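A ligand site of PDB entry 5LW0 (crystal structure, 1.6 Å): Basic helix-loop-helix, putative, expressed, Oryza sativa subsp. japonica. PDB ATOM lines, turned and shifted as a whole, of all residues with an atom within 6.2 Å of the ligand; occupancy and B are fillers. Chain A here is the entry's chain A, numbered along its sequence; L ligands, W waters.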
ATOM      1  N   PRO A  41     -12.076 -11.259  -5.710  1.00  0.00           N
ATOM      2  CA  PRO A  41     -11.914 -12.150  -6.834  1.00  0.00           C
ATOM      3  C   PRO A  41     -12.407 -11.515  -8.131  1.00  0.00           C
ATOM      4  O   PRO A  41     -13.075 -10.451  -8.095  1.00  0.00           O
ATOM      5  CB  PRO A  41     -12.845 -13.281  -6.465  1.00  0.00           C
ATOM      6  CG  PRO A  41     -13.989 -12.569  -5.848  1.00  0.00           C
ATOM      7  CD  PRO A  41     -13.405 -11.361  -5.133  1.00  0.00           C
ATOM      8  N   SER A  42     -12.157 -12.174  -9.257  1.00  0.00           N
ATOM      9  CA  SER A  42     -12.616 -11.688 -10.535  1.00  0.00           C
ATOM     10  C   SER A  42     -14.122 -11.944 -10.672  1.00  0.00           C
ATOM     11  O   SER A  42     -14.563 -13.068 -10.864  1.00  0.00           O
ATOM     12  CB  SER A  42     -11.874 -12.357 -11.627  1.00  0.00           C
ATOM     13  OG  SER A  42     -12.353 -11.963 -12.915  1.00  0.00           O
ATOM     14  N   ILE A  43     -14.886 -10.908 -10.557  1.00  0.00           N
ATOM     15  CA  ILE A  43     -16.340 -11.020 -10.647  1.00  0.00           C
ATOM     16  C   ILE A  43     -16.811 -11.406 -12.024  1.00  0.00           C
ATOM     17  O   ILE A  43     -16.289 -10.905 -13.021  1.00  0.00           O
ATOM     18  CB  ILE A  43     -16.980  -9.635 -10.307  1.00  0.00           C
ATOM     19  CG1 ILE A  43     -16.522  -9.130  -8.920  1.00  0.00           C
ATOM     20  CG2 ILE A  43     -18.500  -9.694 -10.398  1.00  0.00           C
ATOM     21  CD1 ILE A  43     -16.792 -10.081  -7.760  1.00  0.00           C
ATOM     22  N   SER A  44     -17.716 -12.391 -12.063  1.00  0.00           N
ATOM     23  CA  SER A  44     -18.460 -12.807 -13.306  1.00  0.00           C
ATOM     24  C   SER A  44     -17.667 -13.735 -14.236  1.00  0.00           C
ATOM     25  O   SER A  44     -18.222 -14.183 -15.203  1.00  0.00           O
ATOM     26  CB  SER A  44     -18.979 -11.588 -14.120  1.00  0.00           C
ATOM     27  OG  SER A  44     -20.014 -10.919 -13.436  1.00  0.00           O
ATOM     28  N   THR A  45     -16.392 -14.020 -13.966  1.00  0.00           N
ATOM     29  CA  THR A  45     -15.603 -14.752 -14.959  1.00  0.00           C
ATOM     30  C   THR A  45     -15.542 -16.270 -14.818  1.00  0.00           C
ATOM     31  O   THR A  45     -14.821 -16.878 -15.554  1.00  0.00           O
ATOM     32  CB  THR A  45     -14.179 -14.220 -15.096  1.00  0.00           C
ATOM     33  OG1 THR A  45     -13.531 -14.259 -13.842  1.00  0.00           O
ATOM     34  CG2 THR A  45     -14.183 -12.830 -15.576  1.00  0.00           C
ATOM     35  N   ALA A  46     -16.232 -16.856 -13.874  1.00  0.00           N
ATOM     36  CA  ALA A  46     -16.264 -18.356 -13.831  1.00  0.00           C
ATOM     37  C   ALA A  46     -17.686 -18.848 -14.063  1.00  0.00           C
ATOM     38  O   ALA A  46     -18.079 -18.942 -15.195  1.00  0.00           O
ATOM     39  CB  ALA A  46     -15.668 -18.898 -12.556  1.00  0.00           C
ATOM     40  N   ASP A  47     -18.487 -18.951 -13.005  1.00  0.00           N
ATOM     41  CA  ASP A  47     -19.903 -19.378 -13.150  1.00  0.00           C
ATOM     42  C   ASP A  47     -20.686 -18.499 -14.109  1.00  0.00           C
ATOM     43  O   ASP A  47     -21.595 -18.985 -14.839  1.00  0.00           O
ATOM     44  CB  ASP A  47     -20.612 -19.437 -11.747  1.00  0.00           C
ATOM     45  CG  ASP A  47     -20.063 -20.572 -10.812  1.00  0.00           C
ATOM     46  OD1 ASP A  47     -19.429 -21.520 -11.335  1.00  0.00           O
ATOM     47  OD2 ASP A  47     -20.265 -20.504  -9.544  1.00  0.00           O
ATOM     48  N   PHE A  48     -20.415 -17.186 -14.127  1.00  0.00           N
ATOM     49  CA  PHE A  48     -21.166 -16.254 -14.957  1.00  0.00           C
ATOM     50  C   PHE A  48     -20.567 -16.061 -16.409  1.00  0.00           C
ATOM     51  O   PHE A  48     -21.110 -15.299 -17.225  1.00  0.00           O
ATOM     52  CB  PHE A  48     -21.315 -14.872 -14.272  1.00  0.00           C
ATOM     53  CG  PHE A  48     -22.450 -14.769 -13.215  1.00  0.00           C
ATOM     54  CD1 PHE A  48     -23.306 -15.833 -12.954  1.00  0.00           C
ATOM     55  CD2 PHE A  48     -22.658 -13.596 -12.523  1.00  0.00           C
ATOM     56  CE1 PHE A  48     -24.312 -15.740 -11.967  1.00  0.00           C
ATOM     57  CE2 PHE A  48     -23.700 -13.493 -11.589  1.00  0.00           C
ATOM     58  CZ  PHE A  48     -24.487 -14.582 -11.294  1.00  0.00           C
ATOM     59  N   GLN A  49     -19.451 -16.734 -16.682  1.00  0.00           N
ATOM     60  CA  GLN A  49     -18.907 -16.898 -18.039  1.00  0.00           C
ATOM     61  C   GLN A  49     -18.642 -15.608 -18.786  1.00  0.00           C
ATOM     62  O   GLN A  49     -18.603 -15.563 -20.039  1.00  0.00           O
ATOM     63  CB  GLN A  49     -19.833 -17.801 -18.868  1.00  0.00           C
ATOM     64  CG  GLN A  49     -19.906 -19.160 -18.261  1.00  0.00           C
ATOM     65  CD  GLN A  49     -20.786 -20.141 -19.064  1.00  0.00           C
ATOM     66  OE1 GLN A  49     -21.570 -19.756 -19.916  1.00  0.00           O
ATOM     67  NE2 GLN A  49     -20.707 -21.396 -18.666  1.00  0.00           N
ATOM     68  N   PHE A  50     -18.266 -14.566 -18.044  1.00  0.00           N
ATOM     69  CA  PHE A  50     -17.864 -13.340 -18.683  1.00  0.00           C
ATOM     70  C   PHE A  50     -16.507 -13.452 -19.318  1.00  0.00           C
ATOM     71  O   PHE A  50     -15.570 -13.923 -18.702  1.00  0.00           O
ATOM     72  CB  PHE A  50     -17.929 -12.207 -17.670  1.00  0.00           C
ATOM     73  CG  PHE A  50     -17.939 -10.839 -18.263  1.00  0.00           C
ATOM     74  CD1 PHE A  50     -16.816 -10.225 -18.712  1.00  0.00           C
ATOM     75  CD2 PHE A  50     -19.127 -10.081 -18.271  1.00  0.00           C
ATOM     76  CE1 PHE A  50     -16.844  -8.908 -19.181  1.00  0.00           C
ATOM     77  CE2 PHE A  50     -19.161  -8.805 -18.744  1.00  0.00           C
ATOM     78  CZ  PHE A  50     -18.007  -8.187 -19.200  1.00  0.00           C
ATOM     79  N   VAL A  78      -7.418 -11.594  -6.200  1.00  0.00           N
ATOM     80  CA  VAL A  78      -7.024 -12.932  -5.831  1.00  0.00           C
ATOM     81  C   VAL A  78      -7.678 -13.973  -6.720  1.00  0.00           C
ATOM     82  O   VAL A  78      -8.834 -13.825  -7.132  1.00  0.00           O
ATOM     83  CB  VAL A  78      -7.321 -13.235  -4.353  1.00  0.00           C
ATOM     84  CG1 VAL A  78      -6.558 -12.273  -3.462  1.00  0.00           C
ATOM     85  CG2 VAL A  78      -8.817 -13.201  -4.071  1.00  0.00           C
ATOM     86  N   ASP A  79      -6.935 -15.061  -6.983  1.00  0.00           N
ATOM     87  CA  ASP A  79      -7.505 -16.251  -7.645  1.00  0.00           C
ATOM     88  C   ASP A  79      -6.762 -17.457  -7.062  1.00  0.00           C
ATOM     89  O   ASP A  79      -5.631 -17.353  -6.558  1.00  0.00           O
ATOM     90  CB  ASP A  79      -7.414 -16.170  -9.162  1.00  0.00           C
ATOM     91  CG  ASP A  79      -8.439 -17.093  -9.891  1.00  0.00           C
ATOM     92  OD1 ASP A  79      -9.287 -17.687  -9.184  1.00  0.00           O
ATOM     93  OD2 ASP A  79      -8.358 -17.232 -11.187  1.00  0.00           O
ATOM     94  N   LEU A  80      -7.371 -18.617  -7.161  1.00  0.00           N
ATOM     95  CA  LEU A  80      -6.884 -19.799  -6.468  1.00  0.00           C
ATOM     96  C   LEU A  80      -5.624 -20.379  -7.072  1.00  0.00           C
ATOM     97  O   LEU A  80      -4.826 -20.963  -6.368  1.00  0.00           O
ATOM     98  CB  LEU A  80      -7.972 -20.875  -6.511  1.00  0.00           C
ATOM     99  CG  LEU A  80      -9.083 -20.732  -5.539  1.00  0.00           C
ATOM    100  CD1 LEU A  80     -10.216 -21.670  -5.977  1.00  0.00           C
ATOM    101  CD2 LEU A  80      -8.522 -21.091  -4.190  1.00  0.00           C
ATOM    102  N   SER A  84      -3.932 -19.178 -13.173  1.00  0.00           N
ATOM    103  CA  SER A  84      -5.074 -18.280 -13.487  1.00  0.00           C
ATOM    104  C   SER A  84      -4.835 -17.380 -14.685  1.00  0.00           C
ATOM    105  O   SER A  84      -3.952 -16.536 -14.691  1.00  0.00           O
ATOM    106  CB  SER A  84      -5.374 -17.378 -12.304  1.00  0.00           C
ATOM    107  OG  SER A  84      -6.349 -16.477 -12.673  1.00  0.00           O
ATOM    108  N   ILE A  86      -7.031 -15.054 -15.630  1.00  0.00           N
ATOM    109  CA  ILE A  86      -7.414 -13.689 -15.309  1.00  0.00           C
ATOM    110  C   ILE A  86      -6.280 -12.969 -14.548  1.00  0.00           C
ATOM    111  O   ILE A  86      -5.988 -11.804 -14.830  1.00  0.00           O
ATOM    112  CB  ILE A  86      -8.771 -13.619 -14.527  1.00  0.00           C
ATOM    113  CG1 ILE A  86      -9.266 -12.194 -14.474  1.00  0.00           C
ATOM    114  CG2 ILE A  86      -8.650 -14.204 -13.107  1.00  0.00           C
ATOM    115  CD1 ILE A  86      -9.698 -11.630 -15.802  1.00  0.00           C
ATOM    116  N   GLY A 109      -4.153 -17.332  -4.156  1.00  0.00           N
ATOM    117  CA  GLY A 109      -4.582 -17.835  -2.879  1.00  0.00           C
ATOM    118  C   GLY A 109      -6.065 -18.047  -2.779  1.00  0.00           C
ATOM    119  O   GLY A 109      -6.792 -17.682  -3.668  1.00  0.00           O
ATOM    120  N   ASP A 110      -6.454 -18.641  -1.698  1.00  0.00           N
ATOM    121  CA  ASP A 110      -7.854 -18.812  -1.355  1.00  0.00           C
ATOM    122  C   ASP A 110      -8.234 -17.556  -0.550  1.00  0.00           C
ATOM    123  O   ASP A 110      -7.621 -17.238   0.481  1.00  0.00           O
ATOM    124  CB  ASP A 110      -7.984 -20.057  -0.491  1.00  0.00           C
ATOM    125  CG  ASP A 110      -9.416 -20.379  -0.073  1.00  0.00           C
ATOM    126  OD1 ASP A 110     -10.313 -19.533  -0.158  1.00  0.00           O
ATOM    127  OD2 ASP A 110      -9.610 -21.541   0.430  1.00  0.00           O
ATOM    128  N   ILE A 111      -9.249 -16.854  -1.021  1.00  0.00           N
ATOM    129  CA  ILE A 111      -9.708 -15.642  -0.399  1.00  0.00           C
ATOM    130  C   ILE A 111     -10.166 -15.808   1.037  1.00  0.00           C
ATOM    131  O   ILE A 111     -10.277 -14.839   1.770  1.00  0.00           O
ATOM    132  CB  ILE A 111     -10.759 -14.970  -1.289  1.00  0.00           C
ATOM    133  CG1 ILE A 111     -10.754 -13.453  -1.071  1.00  0.00           C
ATOM    134  CG2 ILE A 111     -12.116 -15.576  -1.133  1.00  0.00           C
ATOM    135  CD1 ILE A 111     -11.576 -12.714  -2.107  1.00  0.00           C
ATOM    136  N   THR A 112     -10.511 -17.058   1.428  1.00  0.00           N
ATOM    137  CA  THR A 112     -10.900 -17.353   2.808  1.00  0.00           C
ATOM    138  C   THR A 112      -9.725 -17.828   3.677  1.00  0.00           C
ATOM    139  O   THR A 112      -9.942 -18.117   4.851  1.00  0.00           O
ATOM    140  CB  THR A 112     -11.995 -18.425   2.845  1.00  0.00           C
ATOM    141  OG1 THR A 112     -11.482 -19.688   2.435  1.00  0.00           O
ATOM    142  CG2 THR A 112     -13.126 -18.043   1.932  1.00  0.00           C
ATOM    143  N   ALA A 128     -18.363 -12.885  -4.897  1.00  0.00           N
ATOM    144  CA  ALA A 128     -19.125 -12.884  -6.084  1.00  0.00           C
ATOM    145  C   ALA A 128     -20.443 -13.608  -5.794  1.00  0.00           C
ATOM    146  O   ALA A 128     -20.546 -14.816  -5.851  1.00  0.00           O
ATOM    147  CB  ALA A 128     -18.359 -13.546  -7.225  1.00  0.00           C
ATOM    148  N   ALA A 129     -21.435 -12.803  -5.488  1.00  0.00           N
ATOM    149  CA  ALA A 129     -22.674 -13.290  -4.907  1.00  0.00           C
ATOM    150  C   ALA A 129     -23.639 -13.705  -5.958  1.00  0.00           C
ATOM    151  O   ALA A 129     -23.467 -13.439  -7.158  1.00  0.00           O
ATOM    152  CB  ALA A 129     -23.280 -12.154  -4.042  1.00  0.00           C
ATOM    153  N   ASN A 130     -24.761 -14.319  -5.519  1.00  0.00           N
ATOM    154  CA  ASN A 130     -25.960 -14.413  -6.371  1.00  0.00           C
ATOM    155  C   ASN A 130     -27.056 -13.409  -5.925  1.00  0.00           C
ATOM    156  O   ASN A 130     -26.951 -12.807  -4.853  1.00  0.00           O
ATOM    157  CB  ASN A 130     -26.489 -15.865  -6.357  1.00  0.00           C
ATOM    158  CG  ASN A 130     -26.840 -16.337  -4.980  1.00  0.00           C
ATOM    159  OD1 ASN A 130     -27.754 -15.812  -4.349  1.00  0.00           O
ATOM    160  ND2 ASN A 130     -26.048 -17.281  -4.449  1.00  0.00           N
ATOM    161  N   TRP A 131     -28.065 -13.222  -6.744  1.00  0.00           N
ATOM    162  CA  TRP A 131     -28.959 -12.086  -6.541  1.00  0.00           C
ATOM    163  C   TRP A 131     -29.789 -12.208  -5.275  1.00  0.00           C
ATOM    164  O   TRP A 131     -30.264 -11.233  -4.746  1.00  0.00           O
ATOM    165  CB  TRP A 131     -29.832 -11.841  -7.776  1.00  0.00           C
ATOM    166  CG  TRP A 131     -30.992 -12.818  -8.008  1.00  0.00           C
ATOM    167  CD1 TRP A 131     -30.993 -13.904  -8.812  1.00  0.00           C
ATOM    168  CD2 TRP A 131     -32.348 -12.674  -7.522  1.00  0.00           C
ATOM    169  NE1 TRP A 131     -32.266 -14.455  -8.854  1.00  0.00           N
ATOM    170  CE2 TRP A 131     -33.106 -13.701  -8.086  1.00  0.00           C
ATOM    171  CE3 TRP A 131     -32.997 -11.740  -6.720  1.00  0.00           C
ATOM    172  CZ2 TRP A 131     -34.459 -13.894  -7.791  1.00  0.00           C
ATOM    173  CZ3 TRP A 131     -34.342 -11.912  -6.422  1.00  0.00           C
ATOM    174  CH2 TRP A 131     -35.038 -13.007  -6.936  1.00  0.00           C
ATOM    175  N   LYS A 134     -27.776 -15.864  -1.210  1.00  0.00           N
ATOM    176  CA  LYS A 134     -27.876 -17.143  -0.508  1.00  0.00           C
ATOM    177  C   LYS A 134     -26.526 -17.859  -0.542  1.00  0.00           C
ATOM    178  O   LYS A 134     -25.719 -17.645  -1.469  1.00  0.00           O
ATOM    179  CB  LYS A 134     -28.930 -18.032  -1.187  1.00  0.00           C
ATOM    180  CG  LYS A 134     -30.322 -17.471  -1.170  1.00  0.00           C
ATOM    181  CD  LYS A 134     -30.914 -17.566   0.210  1.00  0.00           C
ATOM    182  CE  LYS A 134     -32.348 -17.011   0.252  1.00  0.00           C
ATOM    183  NZ  LYS A 134     -32.714 -16.647   1.633  1.00  0.00           N
ATOM    184  N   PRO A 135     -26.292 -18.697   0.411  1.00  0.00           N
ATOM    185  CA  PRO A 135     -25.105 -19.557   0.430  1.00  0.00           C
ATOM    186  C   PRO A 135     -25.095 -20.612  -0.622  1.00  0.00           C
ATOM    187  O   PRO A 135     -26.048 -20.770  -1.346  1.00  0.00           O
ATOM    188  CB  PRO A 135     -25.179 -20.260   1.802  1.00  0.00           C
ATOM    189  CG  PRO A 135     -26.297 -19.693   2.509  1.00  0.00           C
ATOM    190  CD  PRO A 135     -27.199 -19.019   1.541  1.00  0.00           C
ATOM    191  N   GLY A 136     -23.984 -21.342  -0.689  1.00  0.00           N
ATOM    192  CA  GLY A 136     -23.861 -22.446  -1.604  1.00  0.00           C
ATOM    193  C   GLY A 136     -23.628 -21.984  -3.013  1.00  0.00           C
ATOM    194  O   GLY A 136     -23.050 -20.892  -3.246  1.00  0.00           O
ATOM    195  N   GLY A 137     -23.979 -22.854  -3.980  1.00  0.00           N
ATOM    196  CA  GLY A 137     -23.885 -22.497  -5.401  1.00  0.00           C
ATOM    197  C   GLY A 137     -22.499 -22.629  -6.004  1.00  0.00           C
ATOM    198  O   GLY A 137     -22.234 -22.089  -7.091  1.00  0.00           O
ATOM    199  N   GLY A 138     -21.594 -23.261  -5.305  1.00  0.00           N
ATOM    200  CA  GLY A 138     -20.228 -23.304  -5.791  1.00  0.00           C
ATOM    201  C   GLY A 138     -19.561 -21.919  -5.909  1.00  0.00           C
ATOM    202  O   GLY A 138     -20.080 -20.897  -5.390  1.00  0.00           O
ATOM    203  N   GLY A 139     -18.389 -21.934  -6.501  1.00  0.00           N
ATOM    204  CA  GLY A 139     -17.560 -20.754  -6.613  1.00  0.00           C
ATOM    205  C   GLY A 139     -17.159 -20.118  -5.300  1.00  0.00           C
ATOM    206  O   GLY A 139     -17.178 -20.715  -4.176  1.00  0.00           O
ATOM    207  N   VAL A 140     -16.783 -18.857  -5.404  1.00  0.00           N
ATOM    208  CA  VAL A 140     -16.277 -18.187  -4.261  1.00  0.00           C
ATOM    209  C   VAL A 140     -17.352 -17.942  -3.246  1.00  0.00           C
ATOM    210  O   VAL A 140     -17.107 -17.952  -2.036  1.00  0.00           O
ATOM    211  CB  VAL A 140     -15.543 -16.883  -4.662  1.00  0.00           C
ATOM    212  CG1 VAL A 140     -16.510 -15.826  -5.067  1.00  0.00           C
ATOM    213  CG2 VAL A 140     -14.707 -16.399  -3.505  1.00  0.00           C
ATOM    214  N   ASN A 141     -18.607 -17.782  -3.697  1.00  0.00           N
ATOM    215  CA  ASN A 141     -19.738 -17.598  -2.764  1.00  0.00           C
ATOM    216  C   ASN A 141     -19.865 -18.781  -1.783  1.00  0.00           C
ATOM    217  O   ASN A 141     -19.952 -18.605  -0.575  1.00  0.00           O
ATOM    218  CB  ASN A 141     -21.003 -17.413  -3.546  1.00  0.00           C
ATOM    219  CG  ASN A 141     -22.197 -17.150  -2.671  1.00  0.00           C
ATOM    220  OD1 ASN A 141     -22.404 -16.081  -2.190  1.00  0.00           O
ATOM    221  ND2 ASN A 141     -23.027 -18.217  -2.469  1.00  0.00           N
ATOM    222  N   ALA A 142     -19.757 -19.996  -2.336  1.00  0.00           N
ATOM    223  CA  ALA A 142     -19.784 -21.181  -1.447  1.00  0.00           C
ATOM    224  C   ALA A 142     -18.666 -21.207  -0.462  1.00  0.00           C
ATOM    225  O   ALA A 142     -18.854 -21.494   0.715  1.00  0.00           O
ATOM    226  CB  ALA A 142     -19.785 -22.436  -2.286  1.00  0.00           C
ATOM    227  N   ALA A 143     -17.463 -20.865  -0.939  1.00  0.00           N
ATOM    228  CA  ALA A 143     -16.301 -20.884  -0.100  1.00  0.00           C
ATOM    229  C   ALA A 143     -16.385 -19.885   1.040  1.00  0.00           C
ATOM    230  O   ALA A 143     -16.018 -20.195   2.144  1.00  0.00           O
ATOM    231  CB  ALA A 143     -15.053 -20.608  -0.952  1.00  0.00           C
ATOM    232  N   ILE A 144     -16.846 -18.640   0.738  1.00  0.00           N
ATOM    233  CA  ILE A 144     -16.954 -17.651   1.725  1.00  0.00           C
ATOM    234  C   ILE A 144     -17.982 -18.011   2.790  1.00  0.00           C
ATOM    235  O   ILE A 144     -17.730 -17.867   3.975  1.00  0.00           O
ATOM    236  CB  ILE A 144     -17.189 -16.223   1.087  1.00  0.00           C
ATOM    237  CG1 ILE A 144     -15.867 -15.783   0.438  1.00  0.00           C
ATOM    238  CG2 ILE A 144     -17.624 -15.266   2.152  1.00  0.00           C
ATOM    239  CD1 ILE A 144     -15.976 -14.554  -0.439  1.00  0.00           C
ATOM    240  N   VAL A 191     -21.026  -8.716  -4.045  1.00  0.00           N
ATOM    241  CA  VAL A 191     -21.094  -8.006  -5.317  1.00  0.00           C
ATOM    242  C   VAL A 191     -21.824  -8.883  -6.329  1.00  0.00           C
ATOM    243  O   VAL A 191     -21.541 -10.098  -6.393  1.00  0.00           O
ATOM    244  CB  VAL A 191     -19.687  -7.785  -5.887  1.00  0.00           C
ATOM    245  CG1 VAL A 191     -19.805  -6.933  -7.111  1.00  0.00           C
ATOM    246  CG2 VAL A 191     -18.781  -7.172  -4.854  1.00  0.00           C
ATOM    247  N   LEU A 192     -22.736  -8.318  -7.085  1.00  0.00           N
ATOM    248  CA  LEU A 192     -23.429  -9.106  -8.146  1.00  0.00           C
ATOM    249  C   LEU A 192     -22.947  -8.572  -9.486  1.00  0.00           C
ATOM    250  O   LEU A 192     -23.248  -7.434  -9.874  1.00  0.00           O
ATOM    251  CB  LEU A 192     -24.927  -8.988  -8.037  1.00  0.00           C
ATOM    252  CG  LEU A 192     -25.685  -9.845  -9.090  1.00  0.00           C
ATOM    253  CD1 LEU A 192     -25.392 -11.301  -8.902  1.00  0.00           C
ATOM    254  CD2 LEU A 192     -27.167  -9.551  -9.005  1.00  0.00           C
ATOM    255  N   GLY A 193     -22.232  -9.413 -10.233  1.00  0.00           N
ATOM    256  CA  GLY A 193     -21.802  -9.009 -11.529  1.00  0.00           C
ATOM    257  C   GLY A 193     -22.829  -9.379 -12.612  1.00  0.00           C
ATOM    258  O   GLY A 193     -23.758 -10.071 -12.304  1.00  0.00           O
ATOM    259  N   PRO A 194     -22.563  -8.987 -13.864  1.00  0.00           N
ATOM    260  CA  PRO A 194     -23.406  -9.433 -14.997  1.00  0.00           C
ATOM    261  C   PRO A 194     -23.265 -10.860 -15.254  1.00  0.00           C
ATOM    262  O   PRO A 194     -22.148 -11.488 -15.070  1.00  0.00           O
ATOM    263  CB  PRO A 194     -22.849  -8.612 -16.164  1.00  0.00           C
ATOM    264  CG  PRO A 194     -21.448  -8.334 -15.812  1.00  0.00           C
ATOM    265  CD  PRO A 194     -21.442  -8.161 -14.314  1.00  0.00           C
ATOM    266  N   ARG A 200     -28.319 -19.166 -15.911  1.00  0.00           N
ATOM    267  CA  ARG A 200     -28.387 -18.371 -14.716  1.00  0.00           C
ATOM    268  C   ARG A 200     -29.276 -17.170 -14.940  1.00  0.00           C
ATOM    269  O   ARG A 200     -29.489 -16.738 -16.089  1.00  0.00           O
ATOM    270  CB  ARG A 200     -26.994 -17.867 -14.304  1.00  0.00           C
ATOM    271  CG  ARG A 200     -25.940 -18.920 -14.073  1.00  0.00           C
ATOM    272  CD  ARG A 200     -26.258 -19.749 -12.855  1.00  0.00           C
ATOM    273  NE  ARG A 200     -25.121 -20.551 -12.493  1.00  0.00           N
ATOM    274  CZ  ARG A 200     -24.330 -20.305 -11.453  1.00  0.00           C
ATOM    275  NH1 ARG A 200     -24.546 -19.263 -10.652  1.00  0.00           N
ATOM    276  NH2 ARG A 200     -23.311 -21.110 -11.212  1.00  0.00           N
HETATM  277  N1  LIG L   1     -10.523 -17.927  -3.480  1.00  0.00           N
HETATM  278  C1  LIG L   1     -10.197 -17.084  -4.484  1.00  0.00           C
HETATM  279  N2  LIG L   1     -10.765 -17.092  -5.674  1.00  0.00           N
HETATM  280  C2  LIG L   1     -11.745 -17.994  -5.964  1.00  0.00           C
HETATM  281  C3  LIG L   1     -12.192 -18.931  -4.970  1.00  0.00           C
HETATM  282  C4  LIG L   1     -11.520 -18.860  -3.663  1.00  0.00           C
HETATM  283  N3  LIG L   1     -11.842 -19.642  -2.664  1.00  0.00           N
HETATM  284  N4  LIG L   1     -13.205 -19.711  -5.564  1.00  0.00           N
HETATM  285  C5  LIG L   1     -13.384 -19.228  -6.807  1.00  0.00           C
HETATM  286  N5  LIG L   1     -12.516 -18.182  -7.068  1.00  0.00           N
HETATM  287  P1  LIG L   1     -17.338 -17.365  -9.302  1.00  0.00           P
HETATM  288  P2  LIG L   1     -19.077 -15.486 -10.830  1.00  0.00           P
HETATM  289  C6  LIG L   1     -12.449 -17.325  -8.225  1.00  0.00           C
HETATM  290  O1  LIG L   1     -17.828 -18.484 -10.242  1.00  0.00           O
HETATM  291  O2  LIG L   1     -18.526 -15.923 -12.171  1.00  0.00           O
HETATM  292  C7  LIG L   1     -21.494 -18.233  -7.333  1.00  0.00           C
HETATM  293  O3  LIG L   1     -21.537 -19.534  -6.778  1.00  0.00           O
HETATM  294  C8  LIG L   1     -12.694 -17.949  -9.593  1.00  0.00           C
HETATM  295  O4  LIG L   1     -11.566 -18.735 -10.077  1.00  0.00           O
HETATM  296  O5  LIG L   1     -17.298 -17.589  -7.836  1.00  0.00           O
HETATM  297  O6  LIG L   1     -19.322 -14.030 -10.570  1.00  0.00           O
HETATM  298  C9  LIG L   1     -22.785 -17.460  -6.925  1.00  0.00           C
HETATM  299  O7  LIG L   1     -23.760 -18.358  -6.247  1.00  0.00           O
HETATM  300  C10 LIG L   1     -13.033 -16.721 -10.400  1.00  0.00           C
HETATM  301  O8  LIG L   1     -11.839 -16.054 -10.909  1.00  0.00           O
HETATM  302  O9  LIG L   1     -18.177 -16.001  -9.587  1.00  0.00           O
HETATM  303  C11 LIG L   1     -23.331 -16.902  -8.214  1.00  0.00           C
HETATM  304  O10 LIG L   1     -24.512 -17.704  -8.523  1.00  0.00           O
HETATM  305  C12 LIG L   1     -13.752 -15.801  -9.394  1.00  0.00           C
HETATM  306  O11 LIG L   1     -13.529 -16.353  -8.113  1.00  0.00           O
HETATM  307  C13 LIG L   1     -22.217 -17.119  -9.253  1.00  0.00           C
HETATM  308  O12 LIG L   1     -21.365 -18.193  -8.789  1.00  0.00           O
HETATM  309  C14 LIG L   1     -15.236 -15.684  -9.627  1.00  0.00           C
HETATM  310  O13 LIG L   1     -15.839 -16.973  -9.858  1.00  0.00           O
HETATM  311  C15 LIG L   1     -21.287 -15.930  -9.466  1.00  0.00           C
HETATM  312  O14 LIG L   1     -20.463 -16.273 -10.602  1.00  0.00           O
HETATM  313  O   HOH W   1     -10.427 -14.321  -9.306  1.00  0.00           O
HETATM  314  O   HOH W   2     -12.333 -22.486  -2.107  1.00  0.00           O
HETATM  315  O   HOH W   3     -16.990 -21.018  -9.962  1.00  0.00           O
HETATM  316  O   HOH W   4     -14.601 -21.363  -9.043  1.00  0.00           O
HETATM  317  O   HOH W   5     -26.695 -17.100  -9.743  1.00  0.00           O
HETATM  318  O   HOH W   6     -21.412 -12.152  -9.046  1.00  0.00           O
HETATM  319  O   HOH W   7     -13.654 -22.048  -4.222  1.00  0.00           O
HETATM  320  O   HOH W   8     -11.777 -16.371 -13.663  1.00  0.00           O
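O of Gly 138 is in hydrogen-bond range of O3 of the ligand. NH1 of Arg 200 lies within hydrogen-bond range of O10 of the ligand, 2.6 Å away. O4 of the ligand is in hydrogen-bond range of OD1 of Asp 79, 2.7 Å away. O of Gly 137 is in hydrogen-bond range of O3 of the ligand (2.7 Å). An oxygen (O1) of the ligand is in hydrogen-bond range of the backbone NH of Asp 47. OD2 of Asp 47 lies within hydrogen-bond range of O3 of the ligand (3.2 Å). O6 of the ligand lies within hydrogen-bond range of N of Ser 44. An oxygen (O5) of the ligand sits at hydrogen-bond distance from the backbone NH of Val 140 (2.8 Å). The side-chain carboxylate of Asp 110 is in hydrogen-bond range of a nitrogen (N3) of the ligand (2.9 Å). The backbone NH of Ile 111 lies within hydrogen-bond range of a nitrogen (N1) of the ligand, at 3.0 Å. The backbone NH (N) of Phe 48 is in hydrogen-bond range of an oxygen (O2) of the ligand (3.0 Å). The backbone NH (N) of Ala 46 sits at hydrogen-bond distance from an oxygen (O2) of the ligand. O7 of the ligand lies within hydrogen-bond range of ND2 of Asn 130 (3.1 Å). An oxygen (O2) of the ligand is in hydrogen-bond range of the backbone NH (N) of Thr 45, 3.4 Å away.
Water W5 lies within hydrogen-bond range of an oxygen (O10) of the ligand (2.6 Å) and the guanidinium group of Arg 200 (3.2 Å). Water W3 lies within hydrogen-bond range of an oxygen (O1) of the ligand (2.7 Å) and the side-chain carboxylate of Asp 47 (2.8 Å). Water W1 lies within hydrogen-bond range of O of Val 78, O8 of the ligand and N of Ser 42. Water W8 bridges OG1 of Thr 45 (2.8 Å) and O8 of the ligand (2.8 Å). Water W6 lies within hydrogen-bond range of the backbone carbonyl oxygen of Ala 129, the backbone NH of Gly 193, an oxygen (O6) of the ligand and the backbone carbonyl oxygen of Val 191.
Residues that only touch the ligand: Pro 41 (3.6 Å), Ser 42 (3.0 Å), Ile 43 (3.9 Å), Leu 80 (3.5 Å), Gly 109 (3.6 Å), Ala 128 (3.4 Å), Ala 129 (3.6 Å), Gly 136 (3.99 Å), Gly 139 (3.4 Å), Asn 141 (3.8 Å) and Ala 143 (3.8 Å). Of the 39 residues printed, 24 come within 4 Å of the ligand. Along chain A the residues within 4 Å of the ligand span positions 41 to 200. The nearest printed residue that does not touch the ligand is Val 78 (4.1 Å).
The side-chain carboxylate of Asp 47 is in salt-bridge range of the guanidinium group of Arg 200. N of Gln 49 lies within hydrogen-bond range of O of Ser 44 (3.2 Å). O of Ser 44 is in hydrogen-bond range of N of Phe 50 (2.9 Å). OD1 of Asp 110 sits at hydrogen-bond distance from OG1 of Thr 112, at 2.8 Å. OG of Ser 42 lies within hydrogen-bond range of OG1 of Thr 45 (2.7 Å). The backbone carbonyl oxygen (O) of Lys 134 lies within hydrogen-bond range of the side-chain amide nitrogen (ND2) of Asn 130 (3.0 Å). N of Ala 129 is in hydrogen-bond range of O of Val 191 (2.9 Å). The side-chain amide nitrogen (ND2) of Asn 141 sits at hydrogen-bond distance from the backbone carbonyl oxygen (O) of Lys 134, at 2.9 Å.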
